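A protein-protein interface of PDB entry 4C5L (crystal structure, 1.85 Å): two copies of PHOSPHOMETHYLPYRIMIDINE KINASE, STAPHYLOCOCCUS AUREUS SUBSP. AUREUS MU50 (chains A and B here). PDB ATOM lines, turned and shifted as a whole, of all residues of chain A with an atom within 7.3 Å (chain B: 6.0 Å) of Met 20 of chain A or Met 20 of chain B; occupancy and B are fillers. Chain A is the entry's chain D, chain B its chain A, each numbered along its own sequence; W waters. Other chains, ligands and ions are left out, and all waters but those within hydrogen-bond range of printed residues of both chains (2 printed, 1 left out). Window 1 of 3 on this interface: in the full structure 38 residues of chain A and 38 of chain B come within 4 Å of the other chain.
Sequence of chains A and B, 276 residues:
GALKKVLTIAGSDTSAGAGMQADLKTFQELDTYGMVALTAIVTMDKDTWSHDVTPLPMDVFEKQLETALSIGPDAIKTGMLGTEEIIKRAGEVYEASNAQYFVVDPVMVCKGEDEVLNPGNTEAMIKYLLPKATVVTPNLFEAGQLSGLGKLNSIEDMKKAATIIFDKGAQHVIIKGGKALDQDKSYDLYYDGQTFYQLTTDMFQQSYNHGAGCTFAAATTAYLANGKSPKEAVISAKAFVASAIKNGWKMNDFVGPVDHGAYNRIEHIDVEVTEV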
ATOM      1  N   THR A   8       8.891  15.633  -9.741  1.00  0.00           N
ATOM      2  CA  THR A   8      10.007  16.045  -8.917  1.00  0.00           C
ATOM      3  C   THR A   8      11.272  15.227  -9.279  1.00  0.00           C
ATOM      4  O   THR A   8      11.191  14.030  -9.554  1.00  0.00           O
ATOM      5  CB  THR A   8       9.644  15.956  -7.437  1.00  0.00           C
ATOM      6  OG1 THR A   8      10.645  16.599  -6.658  1.00  0.00           O
ATOM      7  CG2 THR A   8       9.404  14.557  -6.992  1.00  0.00           C
ATOM      8  N   ILE A   9      12.418  15.923  -9.345  1.00  0.00           N
ATOM      9  CA  ILE A   9      13.736  15.322  -9.585  1.00  0.00           C
ATOM     10  C   ILE A   9      14.402  15.527  -8.249  1.00  0.00           C
ATOM     11  O   ILE A   9      14.790  16.663  -7.903  1.00  0.00           O
ATOM     12  CB  ILE A   9      14.489  16.046 -10.703  1.00  0.00           C
ATOM     13  CG1 ILE A   9      13.694  15.931 -11.987  1.00  0.00           C
ATOM     14  CG2 ILE A   9      15.876  15.446 -10.935  1.00  0.00           C
ATOM     15  CD1 ILE A   9      14.244  16.713 -13.150  1.00  0.00           C
ATOM     16  N   ALA A  10      14.520  14.437  -7.509  1.00  0.00           N
ATOM     17  CA  ALA A  10      14.774  14.503  -6.093  1.00  0.00           C
ATOM     18  C   ALA A  10      15.311  13.207  -5.513  1.00  0.00           C
ATOM     19  O   ALA A  10      15.344  12.187  -6.168  1.00  0.00           O
ATOM     20  CB  ALA A  10      13.504  14.904  -5.371  1.00  0.00           C
ATOM     21  N   GLY A  11      15.722  13.280  -4.259  1.00  0.00           N
ATOM     22  CA  GLY A  11      16.211  12.130  -3.524  1.00  0.00           C
ATOM     23  C   GLY A  11      15.186  11.538  -2.572  1.00  0.00           C
ATOM     24  O   GLY A  11      14.237  12.193  -2.184  1.00  0.00           O
ATOM     25  N   SER A  12      15.368  10.276  -2.217  1.00  0.00           N
ATOM     26  CA  SER A  12      14.454   9.644  -1.285  1.00  0.00           C
ATOM     27  C   SER A  12      14.904   9.927   0.129  1.00  0.00           C
ATOM     28  O   SER A  12      16.020   9.630   0.484  1.00  0.00           O
ATOM     29  CB  SER A  12      14.422   8.138  -1.502  1.00  0.00           C
ATOM     30  OG  SER A  12      13.603   7.500  -0.554  1.00  0.00           O
ATOM     31  N   ASP A  13      14.006  10.470   0.938  1.00  0.00           N
ATOM     32  CA  ASP A  13      14.278  10.636   2.354  1.00  0.00           C
ATOM     33  C   ASP A  13      13.606   9.479   3.083  1.00  0.00           C
ATOM     34  O   ASP A  13      12.416   9.507   3.317  1.00  0.00           O
ATOM     35  CB  ASP A  13      13.734  11.971   2.866  1.00  0.00           C
ATOM     36  CG  ASP A  13      13.595  12.019   4.396  1.00  0.00           C
ATOM     37  OD1 ASP A  13      14.199  11.195   5.076  1.00  0.00           O
ATOM     38  OD2 ASP A  13      12.875  12.884   4.892  1.00  0.00           O
ATOM     39  N   ALA A  16      10.789   9.969   5.397  1.00  0.00           N
ATOM     40  CA  ALA A  16       9.538  10.210   4.674  1.00  0.00           C
ATOM     41  C   ALA A  16       8.902  11.586   4.933  1.00  0.00           C
ATOM     42  O   ALA A  16       7.824  11.889   4.364  1.00  0.00           O
ATOM     43  CB  ALA A  16       8.544   9.073   4.932  1.00  0.00           C
ATOM     44  N   GLY A  17       9.600  12.399   5.716  1.00  0.00           N
ATOM     45  CA  GLY A  17       9.196  13.756   5.995  1.00  0.00           C
ATOM     46  C   GLY A  17       9.587  14.746   4.902  1.00  0.00           C
ATOM     47  O   GLY A  17       8.908  15.715   4.686  1.00  0.00           O
ATOM     48  N   ALA A  18      10.704  14.483   4.246  1.00  0.00           N
ATOM     49  CA  ALA A  18      11.278  15.389   3.277  1.00  0.00           C
ATOM     50  C   ALA A  18      11.459  14.727   1.897  1.00  0.00           C
ATOM     51  O   ALA A  18      10.879  13.700   1.614  1.00  0.00           O
ATOM     52  CB  ALA A  18      12.584  15.959   3.789  1.00  0.00           C
ATOM     53  N   GLY A  19      12.192  15.387   1.025  1.00  0.00           N
ATOM     54  CA  GLY A  19      12.610  14.793  -0.230  1.00  0.00           C
ATOM     55  C   GLY A  19      11.416  14.352  -1.028  1.00  0.00           C
ATOM     56  O   GLY A  19      10.330  14.853  -0.838  1.00  0.00           O
ATOM     57  N   MET A  20      11.591  13.318  -1.826  1.00  0.00           N
ATOM     58  CA  MET A  20      10.556  12.947  -2.778  1.00  0.00           C
ATOM     59  C   MET A  20       9.254  12.578  -2.063  1.00  0.00           C
ATOM     60  O   MET A  20       8.181  12.679  -2.604  1.00  0.00           O
ATOM     61  CB  MET A  20      11.007  11.832  -3.705  1.00  0.00           C
ATOM     62  CG  MET A  20      11.222  10.504  -3.016  1.00  0.00           C
ATOM     63  SD  MET A  20       9.798   9.434  -3.201  1.00  0.00           S
ATOM     64  CE  MET A  20      10.534   7.855  -2.874  1.00  0.00           C
ATOM     65  N   GLN A  21       9.387  12.070  -0.854  1.00  0.00           N
ATOM     66  CA  GLN A  21       8.223  11.709  -0.092  1.00  0.00           C
ATOM     67  C   GLN A  21       7.344  12.906   0.211  1.00  0.00           C
ATOM     68  O   GLN A  21       6.155  12.817   0.156  1.00  0.00           O
ATOM     69  CB  GLN A  21       8.668  11.019   1.199  1.00  0.00           C
ATOM     70  CG  GLN A  21       9.114   9.612   0.924  1.00  0.00           C
ATOM     71  CD  GLN A  21      10.589   9.482   0.601  1.00  0.00           C
ATOM     72  OE1 GLN A  21      11.215  10.411   0.140  1.00  0.00           O
ATOM     73  NE2 GLN A  21      11.137   8.306   0.859  1.00  0.00           N
ATOM     74  N   ALA A  22       7.962  14.007   0.569  1.00  0.00           N
ATOM     75  CA  ALA A  22       7.240  15.227   0.836  1.00  0.00           C
ATOM     76  C   ALA A  22       6.602  15.655  -0.470  1.00  0.00           C
ATOM     77  O   ALA A  22       5.483  16.066  -0.496  1.00  0.00           O
ATOM     78  CB  ALA A  22       8.190  16.303   1.300  1.00  0.00           C
ATOM     79  N   ASP A  23       7.366  15.535  -1.529  1.00  0.00           N
ATOM     80  CA  ASP A  23       6.905  16.054  -2.807  1.00  0.00           C
ATOM     81  C   ASP A  23       5.655  15.313  -3.225  1.00  0.00           C
ATOM     82  O   ASP A  23       4.653  15.914  -3.518  1.00  0.00           O
ATOM     83  CB  ASP A  23       7.993  15.843  -3.831  1.00  0.00           C
ATOM     84  CG  ASP A  23       9.200  16.752  -3.616  1.00  0.00           C
ATOM     85  OD1 ASP A  23       9.078  17.737  -2.888  1.00  0.00           O
ATOM     86  OD2 ASP A  23      10.276  16.438  -4.154  1.00  0.00           O
ATOM     87  N   LEU A  24       5.701  13.995  -3.152  1.00  0.00           N
ATOM     88  CA  LEU A  24       4.596  13.186  -3.626  1.00  0.00           C
ATOM     89  C   LEU A  24       3.356  13.399  -2.774  1.00  0.00           C
ATOM     90  O   LEU A  24       2.262  13.533  -3.273  1.00  0.00           O
ATOM     91  CB  LEU A  24       4.983  11.723  -3.647  1.00  0.00           C
ATOM     92  CG  LEU A  24       6.077  11.322  -4.625  1.00  0.00           C
ATOM     93  CD1 LEU A  24       6.277   9.823  -4.523  1.00  0.00           C
ATOM     94  CD2 LEU A  24       5.643  11.707  -6.025  1.00  0.00           C
ATOM     95  N   LYS A  25       3.569  13.386  -1.461  1.00  0.00           N
ATOM     96  CA  LYS A  25       2.535  13.663  -0.499  1.00  0.00           C
ATOM     97  C   LYS A  25       1.818  14.997  -0.728  1.00  0.00           C
ATOM     98  O   LYS A  25       0.598  15.090  -0.627  1.00  0.00           O
ATOM     99  CB  LYS A  25       3.114  13.621   0.890  1.00  0.00           C
ATOM    100  CG  LYS A  25       3.485  12.209   1.315  1.00  0.00           C
ATOM    101  CD  LYS A  25       4.062  12.169   2.709  1.00  0.00           C
ATOM    102  CE  LYS A  25       4.679  10.843   3.034  1.00  0.00           C
ATOM    103  NZ  LYS A  25       5.007  10.699   4.483  1.00  0.00           N
ATOM    104  N   THR A  26       2.606  16.035  -0.949  1.00  0.00           N
ATOM    105  CA  THR A  26       2.119  17.381  -1.151  1.00  0.00           C
ATOM    106  C   THR A  26       1.433  17.473  -2.469  1.00  0.00           C
ATOM    107  O   THR A  26       0.334  18.069  -2.561  1.00  0.00           O
ATOM    108  CB  THR A  26       3.290  18.388  -1.055  1.00  0.00           C
ATOM    109  OG1 THR A  26       3.812  18.351   0.280  1.00  0.00           O
ATOM    110  CG2 THR A  26       2.843  19.830  -1.431  1.00  0.00           C
ATOM    111  N   PHE A  27       2.016  16.865  -3.498  1.00  0.00           N
ATOM    112  CA  PHE A  27       1.342  16.842  -4.839  1.00  0.00           C
ATOM    113  C   PHE A  27      -0.082  16.218  -4.804  1.00  0.00           C
ATOM    114  O   PHE A  27      -1.001  16.629  -5.539  1.00  0.00           O
ATOM    115  CB  PHE A  27       2.180  16.070  -5.879  1.00  0.00           C
ATOM    116  CG  PHE A  27       3.513  16.699  -6.202  1.00  0.00           C
ATOM    117  CD1 PHE A  27       3.742  18.059  -6.037  1.00  0.00           C
ATOM    118  CD2 PHE A  27       4.559  15.913  -6.655  1.00  0.00           C
ATOM    119  CE1 PHE A  27       4.977  18.619  -6.334  1.00  0.00           C
ATOM    120  CE2 PHE A  27       5.790  16.467  -6.927  1.00  0.00           C
ATOM    121  CZ  PHE A  27       5.998  17.820  -6.804  1.00  0.00           C
ATOM    122  N   MET A  35       4.885  12.568  -9.812  1.00  0.00           N
ATOM    123  CA  MET A  35       5.889  11.652 -10.330  1.00  0.00           C
ATOM    124  C   MET A  35       7.245  12.038  -9.808  1.00  0.00           C
ATOM    125  O   MET A  35       7.459  13.196  -9.427  1.00  0.00           O
ATOM    126  CB  MET A  35       5.961  11.766 -11.841  1.00  0.00           C
ATOM    127  CG  MET A  35       4.699  11.381 -12.535  1.00  0.00           C
ATOM    128  SD  MET A  35       4.909  11.781 -14.269  1.00  0.00           S
ATOM    129  CE  MET A  35       4.637  13.536 -14.175  1.00  0.00           C
ATOM    130  N   VAL A  36       8.172  11.076  -9.809  1.00  0.00           N
ATOM    131  CA  VAL A  36       9.510  11.295  -9.310  1.00  0.00           C
ATOM    132  C   VAL A  36      10.542  10.606 -10.180  1.00  0.00           C
ATOM    133  O   VAL A  36      10.264   9.538 -10.742  1.00  0.00           O
ATOM    134  CB  VAL A  36       9.676  10.879  -7.804  1.00  0.00           C
ATOM    135  CG1 VAL A  36       9.161   9.486  -7.581  1.00  0.00           C
ATOM    136  CG2 VAL A  36      11.125  10.949  -7.335  1.00  0.00           C
ATOM    137  N   ALA A  37      11.689  11.281 -10.325  1.00  0.00           N
ATOM    138  CA  ALA A  37      12.939  10.702 -10.824  1.00  0.00           C
ATOM    139  C   ALA A  37      13.940  10.806  -9.709  1.00  0.00           C
ATOM    140  O   ALA A  37      14.330  11.920  -9.333  1.00  0.00           O
ATOM    141  CB  ALA A  37      13.433  11.471 -12.025  1.00  0.00           C
ATOM    142  N   LEU A  38      14.297   9.656  -9.133  1.00  0.00           N
ATOM    143  CA  LEU A  38      15.148   9.559  -7.973  1.00  0.00           C
ATOM    144  C   LEU A  38      16.614   9.758  -8.373  1.00  0.00           C
ATOM    145  O   LEU A  38      17.100   9.176  -9.324  1.00  0.00           O
ATOM    146  CB  LEU A  38      14.995   8.176  -7.312  1.00  0.00           C
ATOM    147  CG  LEU A  38      13.581   7.740  -6.941  1.00  0.00           C
ATOM    148  CD1 LEU A  38      13.537   6.304  -6.407  1.00  0.00           C
ATOM    149  CD2 LEU A  38      13.021   8.672  -5.883  1.00  0.00           C
ATOM    150  N   ALA A  40      19.000   9.796  -5.670  1.00  0.00           N
ATOM    151  CA  ALA A  40      19.760   9.357  -4.493  1.00  0.00           C
ATOM    152  C   ALA A  40      18.848   8.808  -3.426  1.00  0.00           C
ATOM    153  O   ALA A  40      17.647   9.127  -3.374  1.00  0.00           O
ATOM    154  CB  ALA A  40      20.577  10.502  -3.906  1.00  0.00           C
ATOM    155  N   GLN A  64      14.830   6.787 -15.731  1.00  0.00           N
ATOM    156  CA  GLN A  64      13.693   7.424 -15.100  1.00  0.00           C
ATOM    157  C   GLN A  64      13.260   8.687 -15.833  1.00  0.00           C
ATOM    158  O   GLN A  64      12.066   8.893 -16.080  1.00  0.00           O
ATOM    159  CB  GLN A  64      13.997   7.757 -13.648  1.00  0.00           C
ATOM    160  CG  GLN A  64      14.180   6.534 -12.768  1.00  0.00           C
ATOM    161  CD  GLN A  64      14.618   6.943 -11.373  1.00  0.00           C
ATOM    162  OE1 GLN A  64      13.786   7.215 -10.527  1.00  0.00           O
ATOM    163  NE2 GLN A  64      15.929   7.050 -11.154  1.00  0.00           N
ATOM    164  N   LYS A  77       9.854  20.247 -10.519  1.00  0.00           N
ATOM    165  CA  LYS A  77      10.489  20.686  -9.324  1.00  0.00           C
ATOM    166  C   LYS A  77      11.791  19.906  -9.205  1.00  0.00           C
ATOM    167  O   LYS A  77      11.850  18.770  -9.619  1.00  0.00           O
ATOM    168  CB  LYS A  77       9.605  20.326  -8.162  1.00  0.00           C
ATOM    169  CG  LYS A  77      10.136  20.826  -6.851  1.00  0.00           C
ATOM    170  CD  LYS A  77       9.930  19.917  -5.673  1.00  0.00           C
ATOM    171  CE  LYS A  77      11.046  20.224  -4.723  1.00  0.00           C
ATOM    172  NZ  LYS A  77      11.040  19.571  -3.406  1.00  0.00           N
ATOM    173  N   MET A  80      17.005  17.529  -3.998  1.00  0.00           N
ATOM    174  CA  MET A  80      18.366  17.038  -3.912  1.00  0.00           C
ATOM    175  C   MET A  80      18.835  16.495  -5.264  1.00  0.00           C
ATOM    176  O   MET A  80      18.337  15.451  -5.712  1.00  0.00           O
ATOM    177  CB  MET A  80      18.466  15.933  -2.870  1.00  0.00           C
ATOM    178  CG  MET A  80      19.813  15.256  -2.850  1.00  0.00           C
ATOM    179  SD  MET A  80      19.961  14.123  -1.463  1.00  0.00           S
ATOM    180  CE  MET A  80      19.955  15.249  -0.058  1.00  0.00           C
ATOM    181  N   CYS A 214      11.043  21.224   1.445  1.00  0.00           N
ATOM    182  CA  CYS A 214      10.578  20.477   0.299  1.00  0.00           C
ATOM    183  C   CYS A 214       9.089  20.674   0.122  1.00  0.00           C
ATOM    184  O   CYS A 214       8.605  20.904  -0.969  1.00  0.00           O
ATOM    185  CB  CYS A 214      10.874  19.001   0.511  1.00  0.00           C
ATOM    186  SG  CYS A 214      12.631  18.656   0.735  1.00  0.00           S
ATOM    187  N   THR B   8       5.660   0.769   3.377  1.00  0.00           N
ATOM    188  CA  THR B   8       5.566  -0.126   2.244  1.00  0.00           C
ATOM    189  C   THR B   8       6.985  -0.591   1.838  1.00  0.00           C
ATOM    190  O   THR B   8       7.889   0.213   1.726  1.00  0.00           O
ATOM    191  CB  THR B   8       4.848   0.522   1.070  1.00  0.00           C
ATOM    192  OG1 THR B   8       4.642  -0.433   0.040  1.00  0.00           O
ATOM    193  CG2 THR B   8       5.593   1.753   0.492  1.00  0.00           C
ATOM    194  N   ALA B  10       8.614  -1.862  -1.262  1.00  0.00           N
ATOM    195  CA  ALA B  10       8.165  -1.886  -2.637  1.00  0.00           C
ATOM    196  C   ALA B  10       9.197  -1.263  -3.532  1.00  0.00           C
ATOM    197  O   ALA B  10      10.181  -0.711  -3.066  1.00  0.00           O
ATOM    198  CB  ALA B  10       6.838  -1.136  -2.743  1.00  0.00           C
ATOM    199  N   GLY B  11       8.912  -1.298  -4.830  1.00  0.00           N
ATOM    200  CA  GLY B  11       9.721  -0.642  -5.818  1.00  0.00           C
ATOM    201  C   GLY B  11       9.098   0.635  -6.308  1.00  0.00           C
ATOM    202  O   GLY B  11       7.898   0.930  -6.067  1.00  0.00           O
ATOM    203  N   SER B  12       9.919   1.392  -7.010  1.00  0.00           N
ATOM    204  CA  SER B  12       9.451   2.587  -7.687  1.00  0.00           C
ATOM    205  C   SER B  12       8.931   2.251  -9.068  1.00  0.00           C
ATOM    206  O   SER B  12       9.653   1.712  -9.916  1.00  0.00           O
ATOM    207  CB  SER B  12      10.569   3.613  -7.785  1.00  0.00           C
ATOM    208  OG  SER B  12      10.131   4.709  -8.555  1.00  0.00           O
ATOM    209  N   ASP B  13       7.655   2.569  -9.269  1.00  0.00           N
ATOM    210  CA  ASP B  13       7.051   2.614 -10.576  1.00  0.00           C
ATOM    211  C   ASP B  13       7.244   4.035 -11.113  1.00  0.00           C
ATOM    212  O   ASP B  13       6.469   4.943 -10.813  1.00  0.00           O
ATOM    213  CB  ASP B  13       5.551   2.303 -10.500  1.00  0.00           C
ATOM    214  CG  ASP B  13       4.810   2.736 -11.760  1.00  0.00           C
ATOM    215  OD1 ASP B  13       5.484   2.894 -12.795  1.00  0.00           O
ATOM    216  OD2 ASP B  13       3.581   2.932 -11.711  1.00  0.00           O
ATOM    217  N   ALA B  18       1.514   2.843 -10.003  1.00  0.00           N
ATOM    218  CA  ALA B  18       1.557   1.666  -9.161  1.00  0.00           C
ATOM    219  C   ALA B  18       2.763   1.769  -8.228  1.00  0.00           C
ATOM    220  O   ALA B  18       3.315   2.823  -8.052  1.00  0.00           O
ATOM    221  CB  ALA B  18       1.647   0.426 -10.027  1.00  0.00           C
ATOM    222  N   GLY B  19       3.123   0.671  -7.593  1.00  0.00           N
ATOM    223  CA  GLY B  19       4.352   0.595  -6.791  1.00  0.00           C
ATOM    224  C   GLY B  19       4.294   1.529  -5.613  1.00  0.00           C
ATOM    225  O   GLY B  19       3.190   1.831  -5.086  1.00  0.00           O
ATOM    226  N   MET B  20       5.458   1.988  -5.173  1.00  0.00           N
ATOM    227  CA  MET B  20       5.507   2.858  -4.002  1.00  0.00           C
ATOM    228  C   MET B  20       4.812   4.177  -4.196  1.00  0.00           C
ATOM    229  O   MET B  20       4.279   4.720  -3.253  1.00  0.00           O
ATOM    230  CB  MET B  20       6.924   3.063  -3.515  1.00  0.00           C
ATOM    231  CG  MET B  20       7.796   3.854  -4.442  1.00  0.00           C
ATOM    232  SD  MET B  20       7.804   5.585  -4.004  1.00  0.00           S
ATOM    233  CE  MET B  20       8.889   6.173  -5.294  1.00  0.00           C
ATOM    234  N   GLN B  21       4.747   4.653  -5.434  1.00  0.00           N
ATOM    235  CA  GLN B  21       4.051   5.859  -5.713  1.00  0.00           C
ATOM    236  C   GLN B  21       2.575   5.707  -5.356  1.00  0.00           C
ATOM    237  O   GLN B  21       2.003   6.570  -4.647  1.00  0.00           O
ATOM    238  CB  GLN B  21       4.233   6.261  -7.175  1.00  0.00           C
ATOM    239  CG  GLN B  21       5.612   6.762  -7.566  1.00  0.00           C
ATOM    240  CD  GLN B  21       6.669   5.663  -7.786  1.00  0.00           C
ATOM    241  OE1 GLN B  21       6.471   4.493  -7.449  1.00  0.00           O
ATOM    242  NE2 GLN B  21       7.822   6.067  -8.314  1.00  0.00           N
ATOM    243  N   ALA B  22       1.964   4.607  -5.794  1.00  0.00           N
ATOM    244  CA  ALA B  22       0.552   4.314  -5.469  1.00  0.00           C
ATOM    245  C   ALA B  22       0.349   4.162  -3.992  1.00  0.00           C
ATOM    246  O   ALA B  22      -0.639   4.631  -3.411  1.00  0.00           O
ATOM    247  CB  ALA B  22       0.073   3.061  -6.209  1.00  0.00           C
ATOM    248  N   ASP B  23       1.291   3.521  -3.376  1.00  0.00           N
ATOM    249  CA  ASP B  23       1.233   3.303  -1.938  1.00  0.00           C
ATOM    250  C   ASP B  23       1.222   4.621  -1.152  1.00  0.00           C
ATOM    251  O   ASP B  23       0.269   4.914  -0.415  1.00  0.00           O
ATOM    252  CB  ASP B  23       2.400   2.410  -1.533  1.00  0.00           C
ATOM    253  CG  ASP B  23       2.298   1.012  -2.110  1.00  0.00           C
ATOM    254  OD1 ASP B  23       1.177   0.600  -2.430  1.00  0.00           O
ATOM    255  OD2 ASP B  23       3.324   0.273  -2.207  1.00  0.00           O
ATOM    256  N   LEU B  24       2.228   5.443  -1.361  1.00  0.00           N
ATOM    257  CA  LEU B  24       2.333   6.709  -0.648  1.00  0.00           C
ATOM    258  C   LEU B  24       1.134   7.616  -0.888  1.00  0.00           C
ATOM    259  O   LEU B  24       0.658   8.269   0.045  1.00  0.00           O
ATOM    260  CB  LEU B  24       3.608   7.467  -1.037  1.00  0.00           C
ATOM    261  CG  LEU B  24       4.905   6.766  -0.702  1.00  0.00           C
ATOM    262  CD1 LEU B  24       6.091   7.584  -1.205  1.00  0.00           C
ATOM    263  CD2 LEU B  24       4.957   6.552   0.793  1.00  0.00           C
ATOM    264  N   LYS B  25       0.716   7.720  -2.147  1.00  0.00           N
ATOM    265  CA  LYS B  25      -0.410   8.516  -2.492  1.00  0.00           C
ATOM    266  C   LYS B  25      -1.678   8.032  -1.779  1.00  0.00           C
ATOM    267  O   LYS B  25      -2.489   8.835  -1.304  1.00  0.00           O
ATOM    268  CB  LYS B  25      -0.650   8.465  -4.014  1.00  0.00           C
ATOM    269  CG  LYS B  25       0.423   9.134  -4.851  1.00  0.00           C
ATOM    270  CD  LYS B  25       0.211   8.935  -6.346  1.00  0.00           C
ATOM    271  CE  LYS B  25       1.383   9.484  -7.142  1.00  0.00           C
ATOM    272  NZ  LYS B  25       1.129   9.634  -8.607  1.00  0.00           N
ATOM    273  N   VAL B  36       8.458   4.409   2.741  1.00  0.00           N
ATOM    274  CA  VAL B  36       8.844   3.390   1.770  1.00  0.00           C
ATOM    275  C   VAL B  36      10.295   2.943   1.987  1.00  0.00           C
ATOM    276  O   VAL B  36      11.155   3.768   2.306  1.00  0.00           O
ATOM    277  CB  VAL B  36       8.662   3.861   0.304  1.00  0.00           C
ATOM    278  CG1 VAL B  36       9.289   5.205   0.019  1.00  0.00           C
ATOM    279  CG2 VAL B  36       9.240   2.834  -0.669  1.00  0.00           C
ATOM    280  N   LEU B  38      12.686   1.158  -0.546  1.00  0.00           N
ATOM    281  CA  LEU B  38      12.786   0.922  -1.967  1.00  0.00           C
ATOM    282  C   LEU B  38      13.586  -0.345  -2.218  1.00  0.00           C
ATOM    283  O   LEU B  38      14.680  -0.497  -1.656  1.00  0.00           O
ATOM    284  CB  LEU B  38      13.457   2.111  -2.675  1.00  0.00           C
ATOM    285  CG  LEU B  38      12.711   3.434  -2.563  1.00  0.00           C
ATOM    286  CD1 LEU B  38      13.530   4.617  -3.111  1.00  0.00           C
ATOM    287  CD2 LEU B  38      11.384   3.330  -3.264  1.00  0.00           C
HETATM  288  O   HOH W   1       7.700   8.426 -10.623  1.00  0.00           O
HETATM  289  O   HOH W   2      10.437   6.298   2.993  1.00  0.00           O
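Water W2 bridges the backbone carbonyl oxygen of Val 36 of chain B (2.7 Å) and the side-chain amide nitrogen of Gln 21 of chain A (3.0 Å). Water W1 bridges O of Val 36 of chain A and NE2 of Gln 21 of chain B.
Met 20 of chain A touches just one residue of chain B: Met 20 (3.4 Å). Printed residues of chain A within 4 Å of Met 20 of chain B: Met 20. Of the printed residues of chain B, Leu 38 of chain A touches Leu 38 (3.7 Å). Printed residues of chain A within 4 Å of Gln 21 of chain B: Val 36. Printed residues of chain A within 4 Å of Leu 38 of chain B: Ser 12 and Leu 38. Of the printed residues of chain A, Val 36 of chain B touches Gln 21 (3.7 Å). The nearest residue of chain B that does not touch Met 20 of chain A is Val 36 of chain B (4.1 Å). The nearest residue of chain A that does not touch Met 20 of chain B is Val 36 of chain A (4.03 Å). The nearest printed residue of chain B that does not touch Val 36 of chain A is Met 20 of chain B (4.03 Å).
Hydrophobic or aromatic side chains of chain A that line the printed part of chain B: Met 20, Val 36 and Leu 38. Among the printed residues, 5 pairs touch across the chains.
The backbone carbonyl oxygen (O) of Ala 40 of chain A sits at hydrogen-bond distance from the backbone NH (N) of Ser 12 of chain A (2.8 Å). N of Asp 13 of chain B lies within hydrogen-bond range of OE1 of Gln 21 of chain B (2.9 Å). N of Leu 38 of chain A lies within hydrogen-bond range of OE1 of Gln 64 of chain A, at 2.9 Å. O of Gly 11 of chain B sits at hydrogen-bond distance from N of Met 20 of chain B (2.8 Å). OG of Ser 12 of chain A lies within hydrogen-bond range of NE2 of Gln 21 of chain A. The backbone NH (N) of Met 20 of chain A sits at hydrogen-bond distance from the backbone carbonyl oxygen (O) of Gly 11 of chain A, at 2.9 Å.
Ser 12 of chain A touches Leu 38 of chain B, but with the chains exchanged Leu 38 of chain A does not touch Ser 12 of chain B (4.2 Å). Met 20 of chain B touches its own counterpart, Met 20 of chain A. Gln 21 of chain A touches Val 36 of chain B, and with the chains exchanged Val 36 of chain A touches Gln 21 of chain B. Leu 38 of chain B touches its own counterpart, Leu 38 of chain A.
Among the printed residues, merely in contact across the chains: Ser 12 of chain A with Leu 38 of chain B (3.9 Å), Met 20 of chain A with Met 20 of chain B (3.4 Å), Gln 21 of chain A with Val 36 of chain B (3.7 Å), Val 36 of chain A with Gln 21 of chain B (3.7 Å) and Leu 38 of chain A with Leu 38 of chain B (3.7 Å).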
